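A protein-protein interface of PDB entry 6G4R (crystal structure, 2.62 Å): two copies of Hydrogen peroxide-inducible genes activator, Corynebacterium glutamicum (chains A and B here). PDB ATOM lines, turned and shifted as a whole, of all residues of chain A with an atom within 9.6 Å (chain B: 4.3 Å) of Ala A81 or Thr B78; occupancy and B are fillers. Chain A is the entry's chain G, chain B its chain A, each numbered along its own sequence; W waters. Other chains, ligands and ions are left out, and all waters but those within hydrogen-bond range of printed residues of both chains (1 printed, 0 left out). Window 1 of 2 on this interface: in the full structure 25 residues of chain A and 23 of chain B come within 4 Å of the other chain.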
ATOM      1  N   PRO A   8      20.715 -20.921  36.044  1.00  0.00           N
ATOM      2  CA  PRO A   8      20.997 -20.156  34.826  1.00  0.00           C
ATOM      3  C   PRO A   8      19.908 -19.130  34.551  1.00  0.00           C
ATOM      4  O   PRO A   8      18.769 -19.250  35.004  1.00  0.00           O
ATOM      5  CB  PRO A   8      21.040 -21.228  33.734  1.00  0.00           C
ATOM      6  CG  PRO A   8      20.163 -22.317  34.255  1.00  0.00           C
ATOM      7  CD  PRO A   8      20.338 -22.314  35.751  1.00  0.00           C
ATOM      8  N   THR A   9      20.282 -18.108  33.790  1.00  0.00           N
ATOM      9  CA  THR A   9      19.376 -17.033  33.418  1.00  0.00           C
ATOM     10  C   THR A   9      18.993 -17.165  31.950  1.00  0.00           C
ATOM     11  O   THR A   9      19.641 -17.875  31.176  1.00  0.00           O
ATOM     12  CB  THR A   9      20.006 -15.658  33.672  1.00  0.00           C
ATOM     13  OG1 THR A   9      21.033 -15.414  32.703  1.00  0.00           O
ATOM     14  CG2 THR A   9      20.609 -15.600  35.068  1.00  0.00           C
ATOM     15  N   LEU A  10      17.918 -16.469  31.574  1.00  0.00           N
ATOM     16  CA  LEU A  10      17.469 -16.501  30.186  1.00  0.00           C
ATOM     17  C   LEU A  10      18.516 -15.908  29.251  1.00  0.00           C
ATOM     18  O   LEU A  10      18.757 -16.441  28.162  1.00  0.00           O
ATOM     19  CB  LEU A  10      16.138 -15.763  30.044  1.00  0.00           C
ATOM     20  CG  LEU A  10      14.926 -16.462  30.663  1.00  0.00           C
ATOM     21  CD1 LEU A  10      13.647 -15.713  30.337  1.00  0.00           C
ATOM     22  CD2 LEU A  10      14.842 -17.904  30.187  1.00  0.00           C
ATOM     23  N   LEU A  13      21.124 -18.547  28.616  1.00  0.00           N
ATOM     24  CA  LEU A  13      20.619 -19.598  27.736  1.00  0.00           C
ATOM     25  C   LEU A  13      20.437 -19.088  26.315  1.00  0.00           C
ATOM     26  O   LEU A  13      20.752 -19.789  25.347  1.00  0.00           O
ATOM     27  CB  LEU A  13      19.292 -20.136  28.269  1.00  0.00           C
ATOM     28  CG  LEU A  13      19.308 -20.799  29.643  1.00  0.00           C
ATOM     29  CD1 LEU A  13      17.900 -21.181  30.071  1.00  0.00           C
ATOM     30  CD2 LEU A  13      20.208 -22.012  29.609  1.00  0.00           C
ATOM     31  N   PRO A  73      19.043 -28.888  22.651  1.00  0.00           N
ATOM     32  CA  PRO A  73      17.582 -28.925  22.456  1.00  0.00           C
ATOM     33  C   PRO A  73      16.794 -28.479  23.674  1.00  0.00           C
ATOM     34  O   PRO A  73      15.745 -27.839  23.526  1.00  0.00           O
ATOM     35  CB  PRO A  73      17.312 -30.398  22.111  1.00  0.00           C
ATOM     36  CG  PRO A  73      18.605 -30.912  21.594  1.00  0.00           C
ATOM     37  CD  PRO A  73      19.653 -30.205  22.392  1.00  0.00           C
ATOM     38  N   PHE A  74      17.268 -28.801  24.879  1.00  0.00           N
ATOM     39  CA  PHE A  74      16.560 -28.374  26.081  1.00  0.00           C
ATOM     40  C   PHE A  74      16.642 -26.866  26.268  1.00  0.00           C
ATOM     41  O   PHE A  74      15.700 -26.252  26.781  1.00  0.00           O
ATOM     42  CB  PHE A  74      17.126 -29.096  27.302  1.00  0.00           C
ATOM     43  CG  PHE A  74      17.066 -30.591  27.200  1.00  0.00           C
ATOM     44  CD1 PHE A  74      15.874 -31.266  27.392  1.00  0.00           C
ATOM     45  CD2 PHE A  74      18.206 -31.323  26.907  1.00  0.00           C
ATOM     46  CE1 PHE A  74      15.817 -32.644  27.295  1.00  0.00           C
ATOM     47  CE2 PHE A  74      18.157 -32.700  26.809  1.00  0.00           C
ATOM     48  CZ  PHE A  74      16.961 -33.361  27.004  1.00  0.00           C
ATOM     49  N   ALA A  75      17.756 -26.256  25.859  1.00  0.00           N
ATOM     50  CA  ALA A  75      17.881 -24.806  25.939  1.00  0.00           C
ATOM     51  C   ALA A  75      17.038 -24.111  24.876  1.00  0.00           C
ATOM     52  O   ALA A  75      16.514 -23.018  25.120  1.00  0.00           O
ATOM     53  CB  ALA A  75      19.350 -24.402  25.818  1.00  0.00           C
ATOM     54  N   LYS A  76      16.901 -24.722  23.696  1.00  0.00           N
ATOM     55  CA  LYS A  76      16.099 -24.117  22.637  1.00  0.00           C
ATOM     56  C   LYS A  76      14.614 -24.174  22.971  1.00  0.00           C
ATOM     57  O   LYS A  76      13.867 -23.234  22.674  1.00  0.00           O
ATOM     58  CB  LYS A  76      16.378 -24.811  21.304  1.00  0.00           C
ATOM     59  N   SER A  77      14.165 -25.273  23.582  1.00  0.00           N
ATOM     60  CA  SER A  77      12.774 -25.364  24.013  1.00  0.00           C
ATOM     61  C   SER A  77      12.472 -24.373  25.129  1.00  0.00           C
ATOM     62  O   SER A  77      11.324 -23.937  25.276  1.00  0.00           O
ATOM     63  CB  SER A  77      12.450 -26.788  24.464  1.00  0.00           C
ATOM     64  OG  SER A  77      13.369 -27.239  25.444  1.00  0.00           O
ATOM     65  N   THR A  78      13.482 -24.010  25.925  1.00  0.00           N
ATOM     66  CA  THR A  78      13.287 -22.994  26.955  1.00  0.00           C
ATOM     67  C   THR A  78      12.988 -21.633  26.338  1.00  0.00           C
ATOM     68  O   THR A  78      12.108 -20.908  26.819  1.00  0.00           O
ATOM     69  CB  THR A  78      14.524 -22.915  27.852  1.00  0.00           C
ATOM     70  OG1 THR A  78      14.807 -24.211  28.394  1.00  0.00           O
ATOM     71  CG2 THR A  78      14.295 -21.935  28.994  1.00  0.00           C
ATOM     72  N   LEU A  79      13.706 -21.266  25.273  1.00  0.00           N
ATOM     73  CA  LEU A  79      13.440 -19.993  24.610  1.00  0.00           C
ATOM     74  C   LEU A  79      12.106 -20.018  23.878  1.00  0.00           C
ATOM     75  O   LEU A  79      11.391 -19.010  23.847  1.00  0.00           O
ATOM     76  CB  LEU A  79      14.573 -19.641  23.649  1.00  0.00           C
ATOM     77  CG  LEU A  79      15.947 -19.407  24.274  1.00  0.00           C
ATOM     78  CD1 LEU A  79      16.962 -19.097  23.192  1.00  0.00           C
ATOM     79  CD2 LEU A  79      15.887 -18.285  25.297  1.00  0.00           C
ATOM     80  N   ASP A  80      11.756 -21.158  23.273  1.00  0.00           N
ATOM     81  CA  ASP A  80      10.471 -21.262  22.589  1.00  0.00           C
ATOM     82  C   ASP A  80       9.319 -21.057  23.564  1.00  0.00           C
ATOM     83  O   ASP A  80       8.292 -20.468  23.209  1.00  0.00           O
ATOM     84  CB  ASP A  80      10.355 -22.618  21.893  1.00  0.00           C
ATOM     85  CG  ASP A  80      11.340 -22.773  20.751  1.00  0.00           C
ATOM     86  OD1 ASP A  80      11.731 -21.746  20.158  1.00  0.00           O
ATOM     87  OD2 ASP A  80      11.723 -23.922  20.446  1.00  0.00           O
ATOM     88  N   ALA A  81       9.471 -21.542  24.799  1.00  0.00           N
ATOM     89  CA  ALA A  81       8.459 -21.289  25.818  1.00  0.00           C
ATOM     90  C   ALA A  81       8.461 -19.824  26.236  1.00  0.00           C
ATOM     91  O   ALA A  81       7.398 -19.228  26.445  1.00  0.00           O
ATOM     92  CB  ALA A  81       8.688 -22.196  27.025  1.00  0.00           C
ATOM     93  N   ALA A  82       9.651 -19.228  26.361  1.00  0.00           N
ATOM     94  CA  ALA A  82       9.740 -17.819  26.726  1.00  0.00           C
ATOM     95  C   ALA A  82       9.275 -16.921  25.587  1.00  0.00           C
ATOM     96  O   ALA A  82       8.607 -15.907  25.824  1.00  0.00           O
ATOM     97  CB  ALA A  82      11.171 -17.471  27.137  1.00  0.00           C
ATOM     98  N   GLU A  83       9.626 -17.266  24.345  1.00  0.00           N
ATOM     99  CA  GLU A  83       9.144 -16.487  23.210  1.00  0.00           C
ATOM    100  C   GLU A  83       7.634 -16.616  23.044  1.00  0.00           C
ATOM    101  O   GLU A  83       6.983 -15.680  22.566  1.00  0.00           O
ATOM    102  CB  GLU A  83       9.863 -16.916  21.931  1.00  0.00           C
ATOM    103  N   SER A  84       7.062 -17.758  23.433  1.00  0.00           N
ATOM    104  CA  SER A  84       5.611 -17.907  23.399  1.00  0.00           C
ATOM    105  C   SER A  84       4.945 -17.091  24.500  1.00  0.00           C
ATOM    106  O   SER A  84       3.812 -16.625  24.329  1.00  0.00           O
ATOM    107  CB  SER A  84       5.229 -19.381  23.522  1.00  0.00           C
ATOM    108  OG  SER A  84       5.694 -19.923  24.744  1.00  0.00           O
ATOM    109  N   PHE A  85       5.630 -16.903  25.632  1.00  0.00           N
ATOM    110  CA  PHE A  85       5.071 -16.080  26.697  1.00  0.00           C
ATOM    111  C   PHE A  85       4.973 -14.623  26.266  1.00  0.00           C
ATOM    112  O   PHE A  85       3.960 -13.964  26.522  1.00  0.00           O
ATOM    113  CB  PHE A  85       5.918 -16.211  27.963  1.00  0.00           C
ATOM    114  CG  PHE A  85       5.489 -15.297  29.076  1.00  0.00           C
ATOM    115  CD1 PHE A  85       4.439 -15.642  29.910  1.00  0.00           C
ATOM    116  CD2 PHE A  85       6.144 -14.095  29.294  1.00  0.00           C
ATOM    117  CE1 PHE A  85       4.043 -14.801  30.935  1.00  0.00           C
ATOM    118  CE2 PHE A  85       5.754 -13.251  30.316  1.00  0.00           C
ATOM    119  CZ  PHE A  85       4.703 -13.605  31.138  1.00  0.00           C
ATOM    120  N   LEU A  86       6.009 -14.107  25.599  1.00  0.00           N
ATOM    121  CA  LEU A  86       5.946 -12.737  25.102  1.00  0.00           C
ATOM    122  C   LEU A  86       4.915 -12.598  23.990  1.00  0.00           C
ATOM    123  O   LEU A  86       4.303 -11.534  23.844  1.00  0.00           O
ATOM    124  CB  LEU A  86       7.324 -12.290  24.615  1.00  0.00           C
ATOM    125  N   SER A  87       4.712 -13.655  23.199  1.00  0.00           N
ATOM    126  CA  SER A  87       3.704 -13.610  22.146  1.00  0.00           C
ATOM    127  C   SER A  87       2.303 -13.533  22.738  1.00  0.00           C
ATOM    128  O   SER A  87       1.468 -12.742  22.285  1.00  0.00           O
ATOM    129  CB  SER A  87       3.842 -14.833  21.238  1.00  0.00           C
ATOM    130  OG  SER A  87       5.093 -14.838  20.575  1.00  0.00           O
ATOM    131  N   HIS A  88       2.023 -14.359  23.748  1.00  0.00           N
ATOM    132  CA  HIS A  88       0.725 -14.338  24.410  1.00  0.00           C
ATOM    133  C   HIS A  88       0.590 -13.169  25.375  1.00  0.00           C
ATOM    134  O   HIS A  88      -0.535 -12.748  25.666  1.00  0.00           O
ATOM    135  CB  HIS A  88       0.473 -15.670  25.114  1.00  0.00           C
ATOM    136  CG  HIS A  88       0.346 -16.821  24.167  1.00  0.00           C
ATOM    137  ND1 HIS A  88       1.427 -17.559  23.739  1.00  0.00           N
ATOM    138  CD2 HIS A  88      -0.732 -17.326  23.524  1.00  0.00           C
ATOM    139  CE1 HIS A  88       1.017 -18.491  22.897  1.00  0.00           C
ATOM    140  NE2 HIS A  88      -0.290 -18.370  22.749  1.00  0.00           N
ATOM    141  N   ALA A  89       1.709 -12.639  25.875  1.00  0.00           N
ATOM    142  CA  ALA A  89       1.672 -11.430  26.690  1.00  0.00           C
ATOM    143  C   ALA A  89       1.156 -10.253  25.884  1.00  0.00           C
ATOM    144  O   ALA A  89       0.781  -9.227  26.461  1.00  0.00           O
ATOM    145  CB  ALA A  89       3.054 -11.106  27.257  1.00  0.00           C
ATOM    146  N   LEU B  13       9.418 -14.197  36.466  1.00  0.00           N
ATOM    147  CA  LEU B  13       8.419 -15.239  36.253  1.00  0.00           C
ATOM    148  C   LEU B  13       8.134 -16.023  37.533  1.00  0.00           C
ATOM    149  O   LEU B  13       6.971 -16.326  37.829  1.00  0.00           O
ATOM    150  CB  LEU B  13       8.870 -16.178  35.137  1.00  0.00           C
ATOM    151  CG  LEU B  13       9.017 -15.521  33.762  1.00  0.00           C
ATOM    152  CD1 LEU B  13       9.564 -16.506  32.742  1.00  0.00           C
ATOM    153  CD2 LEU B  13       7.683 -14.958  33.303  1.00  0.00           C
ATOM    154  N   PHE B  74       1.871 -20.386  30.533  1.00  0.00           N
ATOM    155  CA  PHE B  74       3.084 -20.178  29.747  1.00  0.00           C
ATOM    156  C   PHE B  74       4.278 -19.831  30.626  1.00  0.00           C
ATOM    157  O   PHE B  74       5.415 -20.178  30.288  1.00  0.00           O
ATOM    158  CB  PHE B  74       2.858 -19.082  28.705  1.00  0.00           C
ATOM    159  CG  PHE B  74       1.741 -19.378  27.750  1.00  0.00           C
ATOM    160  CD1 PHE B  74       1.921 -20.281  26.715  1.00  0.00           C
ATOM    161  CD2 PHE B  74       0.512 -18.756  27.884  1.00  0.00           C
ATOM    162  CE1 PHE B  74       0.896 -20.558  25.834  1.00  0.00           C
ATOM    163  CE2 PHE B  74      -0.516 -19.028  27.003  1.00  0.00           C
ATOM    164  CZ  PHE B  74      -0.324 -19.930  25.978  1.00  0.00           C
ATOM    165  N   ALA B  75       4.045 -19.150  31.750  1.00  0.00           N
ATOM    166  CA  ALA B  75       5.145 -18.840  32.657  1.00  0.00           C
ATOM    167  C   ALA B  75       5.622 -20.087  33.390  1.00  0.00           C
ATOM    168  O   ALA B  75       6.819 -20.235  33.660  1.00  0.00           O
ATOM    169  CB  ALA B  75       4.720 -17.759  33.648  1.00  0.00           C
ATOM    170  N   LYS B  76       4.701 -20.994  33.723  1.00  0.00           N
ATOM    171  CA  LYS B  76       5.094 -22.219  34.413  1.00  0.00           C
ATOM    172  C   LYS B  76       5.823 -23.173  33.477  1.00  0.00           C
ATOM    173  O   LYS B  76       6.780 -23.841  33.885  1.00  0.00           O
ATOM    174  CB  LYS B  76       3.869 -22.894  35.031  1.00  0.00           C
ATOM    175  CG  LYS B  76       3.189 -22.060  36.105  1.00  0.00           C
ATOM    176  CD  LYS B  76       2.291 -22.906  36.992  1.00  0.00           C
ATOM    177  CE  LYS B  76       1.193 -23.588  36.194  1.00  0.00           C
ATOM    178  NZ  LYS B  76       0.225 -24.289  37.082  1.00  0.00           N
ATOM    179  N   SER B  77       5.386 -23.255  32.216  1.00  0.00           N
ATOM    180  CA  SER B  77       6.093 -24.089  31.249  1.00  0.00           C
ATOM    181  C   SER B  77       7.480 -23.539  30.948  1.00  0.00           C
ATOM    182  O   SER B  77       8.395 -24.307  30.628  1.00  0.00           O
ATOM    183  CB  SER B  77       5.279 -24.215  29.963  1.00  0.00           C
ATOM    184  OG  SER B  77       4.931 -22.940  29.451  1.00  0.00           O
ATOM    185  N   THR B  78       7.654 -22.218  31.038  1.00  0.00           N
ATOM    186  CA  THR B  78       8.983 -21.635  30.886  1.00  0.00           C
ATOM    187  C   THR B  78       9.893 -22.050  32.036  1.00  0.00           C
ATOM    188  O   THR B  78      11.071 -22.361  31.823  1.00  0.00           O
ATOM    189  CB  THR B  78       8.886 -20.111  30.799  1.00  0.00           C
ATOM    190  OG1 THR B  78       7.999 -19.747  29.734  1.00  0.00           O
ATOM    191  CG2 THR B  78      10.255 -19.500  30.541  1.00  0.00           C
ATOM    192  N   LEU B  79       9.363 -22.060  33.261  1.00  0.00           N
ATOM    193  CA  LEU B  79      10.157 -22.481  34.410  1.00  0.00           C
ATOM    194  C   LEU B  79      10.452 -23.974  34.358  1.00  0.00           C
ATOM    195  O   LEU B  79      11.554 -24.407  34.717  1.00  0.00           O
ATOM    196  CB  LEU B  79       9.431 -22.119  35.706  1.00  0.00           C
ATOM    197  CG  LEU B  79       9.193 -20.630  35.964  1.00  0.00           C
ATOM    198  CD1 LEU B  79       8.418 -20.425  37.257  1.00  0.00           C
ATOM    199  CD2 LEU B  79      10.510 -19.873  36.000  1.00  0.00           C
ATOM    200  N   ASP B  80       9.477 -24.777  33.923  1.00  0.00           N
ATOM    201  CA  ASP B  80       9.703 -26.213  33.791  1.00  0.00           C
ATOM    202  C   ASP B  80      10.780 -26.508  32.754  1.00  0.00           C
ATOM    203  O   ASP B  80      11.563 -27.452  32.911  1.00  0.00           O
ATOM    204  CB  ASP B  80       8.397 -26.919  33.425  1.00  0.00           C
ATOM    205  CG  ASP B  80       7.371 -26.862  34.539  1.00  0.00           C
ATOM    206  OD1 ASP B  80       7.774 -26.766  35.717  1.00  0.00           O
ATOM    207  OD2 ASP B  80       6.160 -26.915  34.237  1.00  0.00           O
ATOM    208  N   ALA B  81      10.831 -25.712  31.684  1.00  0.00           N
ATOM    209  CA  ALA B  81      11.874 -25.888  30.678  1.00  0.00           C
ATOM    210  C   ALA B  81      13.240 -25.497  31.227  1.00  0.00           C
ATOM    211  O   ALA B  81      14.245 -26.156  30.934  1.00  0.00           O
ATOM    212  CB  ALA B  81      11.540 -25.075  29.428  1.00  0.00           C
ATOM    213  N   ALA B  82      13.299 -24.429  32.026  1.00  0.00           N
ATOM    214  CA  ALA B  82      14.571 -24.019  32.613  1.00  0.00           C
ATOM    215  C   ALA B  82      15.032 -25.011  33.672  1.00  0.00           C
ATOM    216  O   ALA B  82      16.227 -25.311  33.771  1.00  0.00           O
ATOM    217  CB  ALA B  82      14.447 -22.615  33.204  1.00  0.00           C
HETATM  218  O   HOH W   1      13.765 -27.496  28.423  1.00  0.00           O
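The side-chain hydroxyl of Thr B78 is in hydrogen-bond range of the backbone carbonyl oxygen of Ala A81.
The side-chain hydroxyl (OG1) of Thr A78 is in hydrogen-bond range of the backbone carbonyl oxygen (O) of Ala B81.
The backbone carbonyl oxygen (O) of Phe B74 is in hydrogen-bond range of the side-chain hydroxyl (OG) of Ser B77, 2.9 Å away.
O of Phe B74 sits at hydrogen-bond distance from OG1 of Thr B78, at 2.7 Å.
The side-chain hydroxyl (OG1) of Thr A78 is in hydrogen-bond range of the backbone carbonyl oxygen (O) of Phe A74 (2.8 Å).
The side-chain hydroxyl (OG) of Ser A84 lies within hydrogen-bond range of the backbone carbonyl oxygen (O) of Ala A81 (2.5 Å).
The backbone carbonyl oxygen (O) of Ser A84 lies within hydrogen-bond range of a ring nitrogen (ND1) of His A88 (2.6 Å).
Among the printed residues, merely in contact across the chains: Thr A78 with Ala B82, Ala A82 with Thr B78, Phe A85 with Leu B13, Phe A85 with Phe B74, Phe A85 with Ala B75 and His A88 with Phe B74.
Of chain A, only Ala A81 and Ala A82 come within 4 Å of Thr B78.
No residue of chain A comes within 4 Å of Ser B77.
Of the printed residues of chain B, Thr A78 touches Ala B81 and Ala B82.
Of the printed residues of chain A, Ala B82 touches Thr A78 (3.9 Å).
Of the printed residues of chain B, Phe A85 touches Leu B13 (3.9 Å), Phe B74 (3.97 Å) and Ala B75 (3.98 Å).
Of the printed residues of chain A, Ala B75 touches Phe A85 (3.98 Å).
The nearest residue of chain B that does not touch Ala A81 is Ser B77 (4.2 Å).
The nearest residue of chain A that does not touch Thr B78 is Thr A78 (4.3 Å).
Of the 10 printed residues of chain B, 6 touch a printed residue of chain A.
Printed residues of chain B that touch a printed residue of chain A: Leu B13, Phe B74, Ala B75, Thr B78, Ala B81 and Ala B82.
Thr A78 touches Ala B81, and with the chains exchanged Ala A81 touches Thr B78.
Thr A78 touches Ala B82, and with the chains exchanged Ala A82 touches Thr B78.
Positions printed for both chains: 13, 74, 75, 76, 77, 78, 79, 80, 81 and 82.
Water W1 lies within hydrogen-bond range of the backbone carbonyl oxygen of Phe A74 (2.8 Å), the backbone carbonyl oxygen of Ala B81 (2.9 Å), the side-chain hydroxyl of Ser A77 (3.0 Å) and the side-chain hydroxyl of Thr A78 (3.4 Å).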
